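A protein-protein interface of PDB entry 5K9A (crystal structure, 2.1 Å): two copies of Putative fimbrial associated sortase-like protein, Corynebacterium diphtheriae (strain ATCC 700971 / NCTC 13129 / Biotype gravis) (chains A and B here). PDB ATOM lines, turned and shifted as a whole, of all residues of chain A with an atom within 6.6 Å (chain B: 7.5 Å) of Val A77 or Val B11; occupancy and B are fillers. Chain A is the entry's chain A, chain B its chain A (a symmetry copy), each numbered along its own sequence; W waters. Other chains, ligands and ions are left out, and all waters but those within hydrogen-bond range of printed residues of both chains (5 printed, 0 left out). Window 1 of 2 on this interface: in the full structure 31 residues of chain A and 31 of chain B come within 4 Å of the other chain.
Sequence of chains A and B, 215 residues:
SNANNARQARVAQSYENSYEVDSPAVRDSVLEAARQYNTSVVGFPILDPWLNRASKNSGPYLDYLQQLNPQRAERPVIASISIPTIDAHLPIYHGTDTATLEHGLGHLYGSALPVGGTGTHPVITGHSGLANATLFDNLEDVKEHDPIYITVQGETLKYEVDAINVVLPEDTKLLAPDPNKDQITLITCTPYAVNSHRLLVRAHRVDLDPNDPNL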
ATOM      1  N   LEU A  68       1.747  -8.641   0.064  1.00  0.00           N
ATOM      2  CA  LEU A  68       2.846  -7.903   0.647  1.00  0.00           C
ATOM      3  C   LEU A  68       2.584  -7.558   2.119  1.00  0.00           C
ATOM      4  O   LEU A  68       2.905  -6.434   2.594  1.00  0.00           O
ATOM      5  CB  LEU A  68       3.245  -6.643  -0.163  1.00  0.00           C
ATOM      6  CG  LEU A  68       3.726  -6.975  -1.569  1.00  0.00           C
ATOM      7  CD1 LEU A  68       3.947  -5.677  -2.324  1.00  0.00           C
ATOM      8  CD2 LEU A  68       4.966  -7.812  -1.585  1.00  0.00           C
ATOM      9  N   GLN A  71       2.958 -10.221   7.796  1.00  0.00           N
ATOM     10  CA  GLN A  71       2.691  -9.941   9.228  1.00  0.00           C
ATOM     11  C   GLN A  71       1.227  -9.772   9.551  1.00  0.00           C
ATOM     12  O   GLN A  71       0.860  -9.714  10.726  1.00  0.00           O
ATOM     13  CB  GLN A  71       3.543  -8.745   9.704  1.00  0.00           C
ATOM     14  CG  GLN A  71       3.175  -7.404   9.094  1.00  0.00           C
ATOM     15  CD  GLN A  71       3.830  -7.096   7.738  1.00  0.00           C
ATOM     16  OE1 GLN A  71       4.081  -7.998   6.931  1.00  0.00           O
ATOM     17  NE2 GLN A  71       4.079  -5.796   7.471  1.00  0.00           N
ATOM     18  N   GLU A  74      -2.611  -3.998   9.806  1.00  0.00           N
ATOM     19  CA  GLU A  74      -3.468  -2.988   9.236  1.00  0.00           C
ATOM     20  C   GLU A  74      -2.567  -1.911   8.602  1.00  0.00           C
ATOM     21  O   GLU A  74      -1.665  -1.388   9.236  1.00  0.00           O
ATOM     22  CB  GLU A  74      -4.318  -2.292  10.304  1.00  0.00           C
ATOM     23  CG  GLU A  74      -5.668  -2.942  10.563  1.00  0.00           C
ATOM     24  CD  GLU A  74      -6.332  -2.428  11.847  1.00  0.00           C
ATOM     25  OE1 GLU A  74      -6.475  -1.176  11.947  1.00  0.00           O
ATOM     26  OE2 GLU A  74      -6.683  -3.265  12.742  1.00  0.00           O
ATOM     27  N   ARG A  75      -2.804  -1.580   7.365  1.00  0.00           N
ATOM     28  CA  ARG A  75      -2.042  -0.459   6.746  1.00  0.00           C
ATOM     29  C   ARG A  75      -0.532  -0.562   6.845  1.00  0.00           C
ATOM     30  O   ARG A  75       0.148   0.390   7.107  1.00  0.00           O
ATOM     31  CB  ARG A  75      -2.533   0.868   7.310  1.00  0.00           C
ATOM     32  CG  ARG A  75      -4.026   1.052   7.031  1.00  0.00           C
ATOM     33  CD  ARG A  75      -4.600   2.373   7.586  1.00  0.00           C
ATOM     34  NE  ARG A  75      -5.929   2.619   6.988  1.00  0.00           N
ATOM     35  CZ  ARG A  75      -6.208   3.363   5.897  1.00  0.00           C
ATOM     36  NH1 ARG A  75      -5.288   4.016   5.207  1.00  0.00           N
ATOM     37  NH2 ARG A  75      -7.459   3.465   5.496  1.00  0.00           N
ATOM     38  N   PRO A  76       0.009  -1.732   6.553  1.00  0.00           N
ATOM     39  CA  PRO A  76       1.459  -1.757   6.524  1.00  0.00           C
ATOM     40  C   PRO A  76       2.086  -0.974   5.310  1.00  0.00           C
ATOM     41  O   PRO A  76       1.443  -0.784   4.252  1.00  0.00           O
ATOM     42  CB  PRO A  76       1.753  -3.251   6.309  1.00  0.00           C
ATOM     43  CG  PRO A  76       0.643  -3.684   5.404  1.00  0.00           C
ATOM     44  CD  PRO A  76      -0.590  -2.934   5.949  1.00  0.00           C
ATOM     45  N   VAL A  77       3.340  -0.580   5.490  1.00  0.00           N
ATOM     46  CA  VAL A  77       4.175  -0.155   4.406  1.00  0.00           C
ATOM     47  C   VAL A  77       4.396  -1.391   3.544  1.00  0.00           C
ATOM     48  O   VAL A  77       4.792  -2.429   4.085  1.00  0.00           O
ATOM     49  CB  VAL A  77       5.486   0.360   4.914  1.00  0.00           C
ATOM     50  CG1 VAL A  77       6.397   0.718   3.742  1.00  0.00           C
ATOM     51  CG2 VAL A  77       5.257   1.619   5.784  1.00  0.00           C
ATOM     52  N   ILE A  78       4.136  -1.290   2.235  1.00  0.00           N
ATOM     53  CA  ILE A  78       4.295  -2.420   1.318  1.00  0.00           C
ATOM     54  C   ILE A  78       5.605  -2.395   0.514  1.00  0.00           C
ATOM     55  O   ILE A  78       6.014  -3.419  -0.013  1.00  0.00           O
ATOM     56  CB  ILE A  78       3.084  -2.654   0.379  1.00  0.00           C
ATOM     57  CG1 ILE A  78       2.813  -1.486  -0.549  1.00  0.00           C
ATOM     58  CG2 ILE A  78       1.859  -3.010   1.191  1.00  0.00           C
ATOM     59  CD1 ILE A  78       1.867  -1.860  -1.692  1.00  0.00           C
ATOM     60  N   ALA A  79       6.216  -1.219   0.420  1.00  0.00           N
ATOM     61  CA  ALA A  79       7.443  -0.960  -0.299  1.00  0.00           C
ATOM     62  C   ALA A  79       7.900   0.467  -0.017  1.00  0.00           C
ATOM     63  O   ALA A  79       7.136   1.279   0.505  1.00  0.00           O
ATOM     64  CB  ALA A  79       7.251  -1.116  -1.795  1.00  0.00           C
ATOM     65  N   SER A  80       9.151   0.771  -0.327  1.00  0.00           N
ATOM     66  CA  SER A  80       9.597   2.145  -0.266  1.00  0.00           C
ATOM     67  C   SER A  80      10.140   2.532  -1.610  1.00  0.00           C
ATOM     68  O   SER A  80      10.550   1.672  -2.442  1.00  0.00           O
ATOM     69  CB  SER A  80      10.678   2.330   0.765  1.00  0.00           C
ATOM     70  OG  SER A  80      11.812   1.647   0.382  1.00  0.00           O
ATOM     71  N   LEU A  90      10.186   7.801   0.395  1.00  0.00           N
ATOM     72  CA  LEU A  90       8.844   7.726   0.889  1.00  0.00           C
ATOM     73  C   LEU A  90       8.339   6.319   0.953  1.00  0.00           C
ATOM     74  O   LEU A  90       8.727   5.469   0.142  1.00  0.00           O
ATOM     75  CB  LEU A  90       7.921   8.506  -0.036  1.00  0.00           C
ATOM     76  CG  LEU A  90       8.127  10.034  -0.086  1.00  0.00           C
ATOM     77  CD1 LEU A  90       7.384  10.654  -1.243  1.00  0.00           C
ATOM     78  CD2 LEU A  90       7.779  10.726   1.212  1.00  0.00           C
ATOM     79  N   PRO A  91       7.466   6.070   1.935  1.00  0.00           N
ATOM     80  CA  PRO A  91       6.806   4.771   1.973  1.00  0.00           C
ATOM     81  C   PRO A  91       5.605   4.677   1.072  1.00  0.00           C
ATOM     82  O   PRO A  91       4.919   5.676   0.832  1.00  0.00           O
ATOM     83  CB  PRO A  91       6.362   4.674   3.399  1.00  0.00           C
ATOM     84  CG  PRO A  91       5.964   6.083   3.738  1.00  0.00           C
ATOM     85  CD  PRO A  91       7.007   6.950   3.038  1.00  0.00           C
ATOM     86  N   ILE A  92       5.349   3.467   0.577  1.00  0.00           N
ATOM     87  CA  ILE A  92       4.196   3.128  -0.217  1.00  0.00           C
ATOM     88  C   ILE A  92       3.279   2.202   0.569  1.00  0.00           C
ATOM     89  O   ILE A  92       3.742   1.239   1.179  1.00  0.00           O
ATOM     90  CB  ILE A  92       4.621   2.437  -1.513  1.00  0.00           C
ATOM     91  CG1 ILE A  92       5.580   3.333  -2.288  1.00  0.00           C
ATOM     92  CG2 ILE A  92       3.419   2.110  -2.395  1.00  0.00           C
ATOM     93  CD1 ILE A  92       6.318   2.611  -3.399  1.00  0.00           C
ATOM     94  N   TYR A  93       1.987   2.477   0.527  1.00  0.00           N
ATOM     95  CA  TYR A  93       0.981   1.741   1.199  1.00  0.00           C
ATOM     96  C   TYR A  93       0.007   1.116   0.200  1.00  0.00           C
ATOM     97  O   TYR A  93      -0.062   1.572  -0.912  1.00  0.00           O
ATOM     98  CB  TYR A  93       0.182   2.665   2.113  1.00  0.00           C
ATOM     99  CG  TYR A  93       0.962   3.249   3.257  1.00  0.00           C
ATOM    100  CD1 TYR A  93       1.149   2.531   4.426  1.00  0.00           C
ATOM    101  CD2 TYR A  93       1.614   4.424   3.123  1.00  0.00           C
ATOM    102  CE1 TYR A  93       1.893   3.058   5.503  1.00  0.00           C
ATOM    103  CE2 TYR A  93       2.349   4.966   4.170  1.00  0.00           C
ATOM    104  CZ  TYR A  93       2.523   4.264   5.330  1.00  0.00           C
ATOM    105  OH  TYR A  93       3.264   4.825   6.296  1.00  0.00           O
ATOM    106  N   HIS A  94      -0.811   0.131   0.620  1.00  0.00           N
ATOM    107  CA  HIS A  94      -1.895  -0.316  -0.220  1.00  0.00           C
ATOM    108  C   HIS A  94      -2.942   0.799  -0.447  1.00  0.00           C
ATOM    109  O   HIS A  94      -3.335   1.502   0.476  1.00  0.00           O
ATOM    110  CB  HIS A  94      -2.727  -1.403   0.465  1.00  0.00           C
ATOM    111  CG  HIS A  94      -2.053  -2.717   0.631  1.00  0.00           C
ATOM    112  ND1 HIS A  94      -1.566  -3.149   1.849  1.00  0.00           N
ATOM    113  CD2 HIS A  94      -1.878  -3.752  -0.238  1.00  0.00           C
ATOM    114  CE1 HIS A  94      -1.091  -4.380   1.711  1.00  0.00           C
ATOM    115  NE2 HIS A  94      -1.268  -4.756   0.462  1.00  0.00           N
ATOM    116  N   HIS A 103      -0.220  10.460   4.422  1.00  0.00           N
ATOM    117  CA  HIS A 103       0.951  10.012   5.196  1.00  0.00           C
ATOM    118  C   HIS A 103       2.019   9.352   4.345  1.00  0.00           C
ATOM    119  O   HIS A 103       3.057   8.974   4.834  1.00  0.00           O
ATOM    120  CB  HIS A 103       0.493   9.074   6.351  1.00  0.00           C
ATOM    121  CG  HIS A 103      -0.524   9.712   7.241  1.00  0.00           C
ATOM    122  ND1 HIS A 103      -0.277  10.896   7.914  1.00  0.00           N
ATOM    123  CD2 HIS A 103      -1.813   9.385   7.517  1.00  0.00           C
ATOM    124  CE1 HIS A 103      -1.354  11.246   8.595  1.00  0.00           C
ATOM    125  NE2 HIS A 103      -2.303  10.354   8.359  1.00  0.00           N
ATOM    126  N   GLN A 153      10.343  -6.206   0.410  1.00  0.00           N
ATOM    127  CA  GLN A 153      10.696  -7.525   1.021  1.00  0.00           C
ATOM    128  C   GLN A 153      12.171  -7.774   0.977  1.00  0.00           C
ATOM    129  O   GLN A 153      12.611  -8.896   0.721  1.00  0.00           O
ATOM    130  CB  GLN A 153       9.947  -8.676   0.337  1.00  0.00           C
ATOM    131  CG  GLN A 153       8.452  -8.601   0.529  1.00  0.00           C
ATOM    132  CD  GLN A 153       8.076  -9.003   1.924  1.00  0.00           C
ATOM    133  OE1 GLN A 153       8.535 -10.043   2.414  1.00  0.00           O
ATOM    134  NE2 GLN A 153       7.206  -8.231   2.561  1.00  0.00           N
ATOM    135  N   ASN B   5       7.926  15.618   6.804  1.00  0.00           N
ATOM    136  CA  ASN B   5       8.753  15.066   5.756  1.00  0.00           C
ATOM    137  C   ASN B   5       9.769  14.126   6.347  1.00  0.00           C
ATOM    138  O   ASN B   5       9.941  12.998   5.884  1.00  0.00           O
ATOM    139  CB  ASN B   5       9.469  16.134   4.955  1.00  0.00           C
ATOM    140  CG  ASN B   5       8.515  16.952   4.110  1.00  0.00           C
ATOM    141  OD1 ASN B   5       7.418  16.527   3.774  1.00  0.00           O
ATOM    142  ND2 ASN B   5       8.935  18.160   3.770  1.00  0.00           N
ATOM    143  N   ALA B   6      10.427  14.579   7.397  1.00  0.00           N
ATOM    144  CA  ALA B   6      11.395  13.747   8.054  1.00  0.00           C
ATOM    145  C   ALA B   6      10.730  12.497   8.617  1.00  0.00           C
ATOM    146  O   ALA B   6      11.329  11.430   8.513  1.00  0.00           O
ATOM    147  CB  ALA B   6      12.116  14.512   9.136  1.00  0.00           C
ATOM    148  N   ARG B   7       9.558  12.623   9.209  1.00  0.00           N
ATOM    149  CA  ARG B   7       8.832  11.480   9.711  1.00  0.00           C
ATOM    150  C   ARG B   7       8.511  10.429   8.610  1.00  0.00           C
ATOM    151  O   ARG B   7       8.693   9.252   8.816  1.00  0.00           O
ATOM    152  CB  ARG B   7       7.548  11.926  10.399  1.00  0.00           C
ATOM    153  CG  ARG B   7       6.779  10.815  11.070  1.00  0.00           C
ATOM    154  CD  ARG B   7       5.913  11.216  12.322  1.00  0.00           C
ATOM    155  NE  ARG B   7       5.125  12.383  12.065  1.00  0.00           N
ATOM    156  CZ  ARG B   7       5.361  13.592  12.545  1.00  0.00           C
ATOM    157  NH1 ARG B   7       6.347  13.816  13.391  1.00  0.00           N
ATOM    158  NH2 ARG B   7       4.589  14.591  12.161  1.00  0.00           N
ATOM    159  N   GLN B   8       8.058  10.900   7.451  1.00  0.00           N
ATOM    160  CA  GLN B   8       7.762  10.018   6.308  1.00  0.00           C
ATOM    161  C   GLN B   8       8.989   9.335   5.786  1.00  0.00           C
ATOM    162  O   GLN B   8       8.937   8.106   5.605  1.00  0.00           O
ATOM    163  CB  GLN B   8       7.019  10.763   5.243  1.00  0.00           C
ATOM    164  CG  GLN B   8       5.649  11.111   5.761  1.00  0.00           C
ATOM    165  CD  GLN B   8       4.910  12.018   4.811  1.00  0.00           C
ATOM    166  OE1 GLN B   8       5.423  12.370   3.769  1.00  0.00           O
ATOM    167  NE2 GLN B   8       3.707  12.413   5.192  1.00  0.00           N
ATOM    168  N   ALA B   9      10.098  10.065   5.637  1.00  0.00           N
ATOM    169  CA  ALA B   9      11.349   9.505   5.235  1.00  0.00           C
ATOM    170  C   ALA B   9      11.876   8.450   6.218  1.00  0.00           C
ATOM    171  O   ALA B   9      12.438   7.400   5.816  1.00  0.00           O
ATOM    172  CB  ALA B   9      12.396  10.582   5.062  1.00  0.00           C
ATOM    173  N   ARG B  10      11.701   8.688   7.523  1.00  0.00           N
ATOM    174  CA  ARG B  10      12.125   7.751   8.493  1.00  0.00           C
ATOM    175  C   ARG B  10      11.259   6.457   8.472  1.00  0.00           C
ATOM    176  O   ARG B  10      11.771   5.382   8.722  1.00  0.00           O
ATOM    177  CB  ARG B  10      12.120   8.404   9.887  1.00  0.00           C
ATOM    178  CG  ARG B  10      12.726   7.507  10.953  1.00  0.00           C
ATOM    179  CD  ARG B  10      12.943   8.257  12.268  1.00  0.00           C
ATOM    180  NE  ARG B  10      13.748   7.453  13.195  1.00  0.00           N
ATOM    181  CZ  ARG B  10      13.960   7.733  14.485  1.00  0.00           C
ATOM    182  NH1 ARG B  10      14.698   6.906  15.206  1.00  0.00           N
ATOM    183  NH2 ARG B  10      13.421   8.807  15.060  1.00  0.00           N
ATOM    184  N   VAL B  11       9.953   6.572   8.237  1.00  0.00           N
ATOM    185  CA  VAL B  11       9.097   5.401   8.014  1.00  0.00           C
ATOM    186  C   VAL B  11       9.635   4.525   6.855  1.00  0.00           C
ATOM    187  O   VAL B  11       9.783   3.314   6.990  1.00  0.00           O
ATOM    188  CB  VAL B  11       7.649   5.766   7.746  1.00  0.00           C
ATOM    189  CG1 VAL B  11       6.804   4.568   7.309  1.00  0.00           C
ATOM    190  CG2 VAL B  11       7.027   6.319   9.053  1.00  0.00           C
ATOM    191  N   ALA B  12      10.016   5.154   5.757  1.00  0.00           N
ATOM    192  CA  ALA B  12      10.635   4.445   4.651  1.00  0.00           C
ATOM    193  C   ALA B  12      11.927   3.802   5.021  1.00  0.00           C
ATOM    194  O   ALA B  12      12.145   2.617   4.722  1.00  0.00           O
ATOM    195  CB  ALA B  12      10.797   5.349   3.467  1.00  0.00           C
ATOM    196  N   GLN B  13      12.824   4.565   5.648  1.00  0.00           N
ATOM    197  CA  GLN B  13      14.117   4.028   6.029  1.00  0.00           C
ATOM    198  C   GLN B  13      13.986   2.866   7.028  1.00  0.00           C
ATOM    199  O   GLN B  13      14.710   1.890   6.891  1.00  0.00           O
ATOM    200  CB  GLN B  13      14.990   5.099   6.691  1.00  0.00           C
ATOM    201  CG  GLN B  13      16.376   4.633   7.010  1.00  0.00           C
ATOM    202  CD  GLN B  13      17.146   4.300   5.727  1.00  0.00           C
ATOM    203  OE1 GLN B  13      17.128   5.068   4.770  1.00  0.00           O
ATOM    204  NE2 GLN B  13      17.718   3.108   5.665  1.00  0.00           N
ATOM    205  N   SER B  14      13.119   2.964   8.022  1.00  0.00           N
ATOM    206  CA  SER B  14      12.954   1.849   8.952  1.00  0.00           C
ATOM    207  C   SER B  14      12.325   0.600   8.348  1.00  0.00           C
ATOM    208  O   SER B  14      12.726  -0.522   8.724  1.00  0.00           O
ATOM    209  CB  SER B  14      12.272   2.236  10.273  1.00  0.00           C
ATOM    210  OG  SER B  14      11.000   2.780  10.035  1.00  0.00           O
ATOM    211  N   TYR B  15      11.394   0.759   7.407  1.00  0.00           N
ATOM    212  CA  TYR B  15      10.924  -0.368   6.584  1.00  0.00           C
ATOM    213  C   TYR B  15      12.117  -1.060   5.911  1.00  0.00           C
ATOM    214  O   TYR B  15      12.247  -2.272   5.994  1.00  0.00           O
ATOM    215  CB  TYR B  15       9.923   0.096   5.479  1.00  0.00           C
ATOM    216  CG  TYR B  15       9.590  -0.969   4.463  1.00  0.00           C
ATOM    217  CD1 TYR B  15       8.651  -1.951   4.763  1.00  0.00           C
ATOM    218  CD2 TYR B  15      10.267  -1.066   3.247  1.00  0.00           C
ATOM    219  CE1 TYR B  15       8.373  -2.975   3.853  1.00  0.00           C
ATOM    220  CE2 TYR B  15       9.990  -2.099   2.315  1.00  0.00           C
ATOM    221  CZ  TYR B  15       9.064  -3.070   2.644  1.00  0.00           C
ATOM    222  OH  TYR B  15       8.726  -4.122   1.781  1.00  0.00           O
ATOM    223  N   GLU B  16      12.960  -0.322   5.208  1.00  0.00           N
ATOM    224  CA  GLU B  16      14.147  -0.888   4.614  1.00  0.00           C
ATOM    225  C   GLU B  16      15.082  -1.544   5.645  1.00  0.00           C
ATOM    226  O   GLU B  16      15.577  -2.648   5.395  1.00  0.00           O
ATOM    227  CB  GLU B  16      14.955   0.167   3.841  1.00  0.00           C
ATOM    228  CG  GLU B  16      14.153   0.720   2.649  1.00  0.00           C
ATOM    229  CD  GLU B  16      14.673   2.050   2.050  1.00  0.00           C
ATOM    230  OE1 GLU B  16      15.789   2.472   2.445  1.00  0.00           O
ATOM    231  OE2 GLU B  16      13.923   2.668   1.206  1.00  0.00           O
ATOM    232  N   ASN B  17      15.379  -0.867   6.758  1.00  0.00           N
ATOM    233  CA  ASN B  17      16.269  -1.417   7.779  1.00  0.00           C
ATOM    234  C   ASN B  17      15.707  -2.734   8.312  1.00  0.00           C
ATOM    235  O   ASN B  17      16.462  -3.573   8.736  1.00  0.00           O
ATOM    236  CB  ASN B  17      16.404  -0.481   8.998  1.00  0.00           C
ATOM    237  CG  ASN B  17      17.096   0.832   8.682  1.00  0.00           C
ATOM    238  OD1 ASN B  17      17.777   0.977   7.664  1.00  0.00           O
ATOM    239  ND2 ASN B  17      16.901   1.818   9.551  1.00  0.00           N
ATOM    240  N   TYR B  19      14.413  -5.309   7.067  1.00  0.00           N
ATOM    241  CA  TYR B  19      14.877  -6.492   6.327  1.00  0.00           C
ATOM    242  C   TYR B  19      16.359  -6.741   6.517  1.00  0.00           C
ATOM    243  O   TYR B  19      16.822  -7.797   6.184  1.00  0.00           O
ATOM    244  CB  TYR B  19      14.478  -6.471   4.841  1.00  0.00           C
ATOM    245  CG  TYR B  19      12.999  -6.467   4.742  1.00  0.00           C
ATOM    246  CD1 TYR B  19      12.263  -7.638   4.827  1.00  0.00           C
ATOM    247  CD2 TYR B  19      12.304  -5.275   4.692  1.00  0.00           C
ATOM    248  CE1 TYR B  19      10.881  -7.622   4.812  1.00  0.00           C
ATOM    249  CE2 TYR B  19      10.917  -5.247   4.700  1.00  0.00           C
ATOM    250  CZ  TYR B  19      10.210  -6.422   4.728  1.00  0.00           C
ATOM    251  OH  TYR B  19       8.846  -6.352   4.773  1.00  0.00           O
ATOM    252  N   GLN B  71      15.610  -1.377  13.891  1.00  0.00           N
ATOM    253  CA  GLN B  71      15.117  -0.709  12.662  1.00  0.00           C
ATOM    254  C   GLN B  71      15.239   0.795  12.697  1.00  0.00           C
ATOM    255  O   GLN B  71      15.033   1.452  11.675  1.00  0.00           O
ATOM    256  CB  GLN B  71      13.681  -1.177  12.342  1.00  0.00           C
ATOM    257  CG  GLN B  71      12.620  -0.736  13.334  1.00  0.00           C
ATOM    258  CD  GLN B  71      12.447  -1.646  14.561  1.00  0.00           C
ATOM    259  OE1 GLN B  71      13.408  -2.255  15.044  1.00  0.00           O
ATOM    260  NE2 GLN B  71      11.207  -1.711  15.092  1.00  0.00           N
ATOM    261  N   ARG B  72      15.550   1.358  13.859  1.00  0.00           N
ATOM    262  CA  ARG B  72      15.575   2.816  14.065  1.00  0.00           C
ATOM    263  C   ARG B  72      14.292   3.547  13.702  1.00  0.00           C
ATOM    264  O   ARG B  72      14.316   4.567  12.987  1.00  0.00           O
ATOM    265  CB  ARG B  72      16.732   3.482  13.282  1.00  0.00           C
ATOM    266  CG  ARG B  72      18.128   2.954  13.591  1.00  0.00           C
ATOM    267  CD  ARG B  72      18.266   2.975  15.079  1.00  0.00           C
ATOM    268  NE  ARG B  72      19.631   2.871  15.586  1.00  0.00           N
ATOM    269  CZ  ARG B  72      19.950   2.196  16.704  1.00  0.00           C
ATOM    270  NH1 ARG B  72      18.983   1.535  17.441  1.00  0.00           N
ATOM    271  NH2 ARG B  72      21.218   2.211  17.080  1.00  0.00           N
ATOM    272  N   ALA B  73      13.167   3.013  14.112  1.00  0.00           N
ATOM    273  CA  ALA B  73      11.917   3.662  13.908  1.00  0.00           C
ATOM    274  C   ALA B  73      11.589   4.704  15.007  1.00  0.00           C
ATOM    275  O   ALA B  73      12.184   4.677  16.095  1.00  0.00           O
ATOM    276  CB  ALA B  73      10.827   2.613  13.849  1.00  0.00           C
ATOM    277  N   GLU B  74      10.618   5.565  14.702  1.00  0.00           N
ATOM    278  CA  GLU B  74       9.979   6.420  15.672  1.00  0.00           C
ATOM    279  C   GLU B  74       8.871   5.602  16.361  1.00  0.00           C
ATOM    280  O   GLU B  74       8.031   5.002  15.711  1.00  0.00           O
ATOM    281  CB  GLU B  74       9.303   7.626  15.012  1.00  0.00           C
ATOM    282  CG  GLU B  74      10.190   8.855  14.877  1.00  0.00           C
ATOM    283  CD  GLU B  74       9.598   9.905  13.928  1.00  0.00           C
ATOM    284  OE1 GLU B  74       8.422  10.296  14.180  1.00  0.00           O
ATOM    285  OE2 GLU B  74      10.294  10.311  12.940  1.00  0.00           O
HETATM  286  O   HOH W   1      13.791   2.407  -1.904  1.00  0.00           O
HETATM  287  O   HOH W   2       6.695  -7.883   5.619  1.00  0.00           O
HETATM  288  O   HOH W   3       6.587  -5.441   1.765  1.00  0.00           O
HETATM  289  O   HOH W   4       7.385  -4.766   7.059  1.00  0.00           O
HETATM  290  O   HOH W   5       3.030  11.676   8.261  1.00  0.00           O
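Val A77 touches just these residues of chain B: Val B11 and Tyr B15. Val B11 touches just these residues of chain A: Val A77, Pro A91 and Tyr A93. Printed residues of chain B within 4 Å of Pro A91: Gln B8 (3.4 Å), Val B11 (3.9 Å) and Ala B12 (3.7 Å). Printed residues of chain A within 4 Å of Tyr B15: Val A77, Ile A78, Ala A79, Ser A80 and Gln A153.
Among the printed residues, merely in contact across the chains: Pro A91 with Gln B8 (3.4 Å), His A103 with Gln B8 (3.5 Å), Val A77 with Tyr B15 (3.6 Å), Leu A90 with Ala B12 (3.6 Å), Val A77 with Val B11 (3.7 Å), Tyr A93 with Val B11 (3.7 Å), Pro A91 with Ala B12 (3.7 Å), Ala A79 with Tyr B15 (3.8 Å), Leu A90 with Gln B8 (3.8 Å), Pro A91 with Val B11 (3.9 Å) and Ser A80 with Tyr B15 (3.99 Å).
Printed residues of chain A that touch a printed residue of chain B: Val A77, Ile A78, Ala A79, Ser A80, Leu A90, Pro A91, Tyr A93, His A103 and Gln A153. Hydrophobic or aromatic side chains of chain A that line the printed part of chain B: Val A77, Leu A90, Pro A91 and Tyr A93. Among the printed residues, 15 pairs touch across the chains. Among the printed residues, no Asp or Glu carboxylate lies within 4 Å of a Lys or Arg side-chain nitrogen of the other chain.
The side-chain hydroxyl (OG) of Ser A80 sits at hydrogen-bond distance from the side-chain carboxylate (OE2) of Glu B16, 2.5 Å away. OH of Tyr B19 lies within hydrogen-bond range of NE2 of Gln A153 (3.3 Å). OH of Tyr B15 lies within hydrogen-bond range of O of Ile A78 (3.3 Å). OH of Tyr B15 lies within hydrogen-bond range of N of Gln A153, at 3.0 Å.
2 positions are printed for both chains.
Water W3 lies within hydrogen-bond range of the side-chain hydroxyl (OH) of Tyr B15, the backbone carbonyl oxygen (O) of Ile A78 and the side-chain amide nitrogen (NE2) of Gln A153. Water W2 lies within hydrogen-bond range of OH of Tyr B19 (2.8 Å), OE1 of Gln A71 (2.9 Å) and NE2 of Gln A153 (3.1 Å). Water W1 bridges the side-chain hydroxyl (OG) of Ser A80 (3.1 Å) and the side-chain carboxylate (OE2) of Glu B16 (3.1 Å). Water W4 bridges the side-chain hydroxyl of Tyr B19 (3.1 Å) and the side-chain amide nitrogen of Gln A71 (3.5 Å). Water W5 lies within hydrogen-bond range of the side-chain amide nitrogen (NE2) of Gln B8 (3.2 Å) and a ring nitrogen (ND1) of His A103 (3.4 Å).
N of Ile A78 lies within hydrogen-bond range of O of Ile A92. O of Val B11 sits at hydrogen-bond distance from OG of Ser B14 (3.3 Å). The backbone carbonyl oxygen of Ala A79 sits at hydrogen-bond distance from the backbone NH of Ile A92 (2.8 Å).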
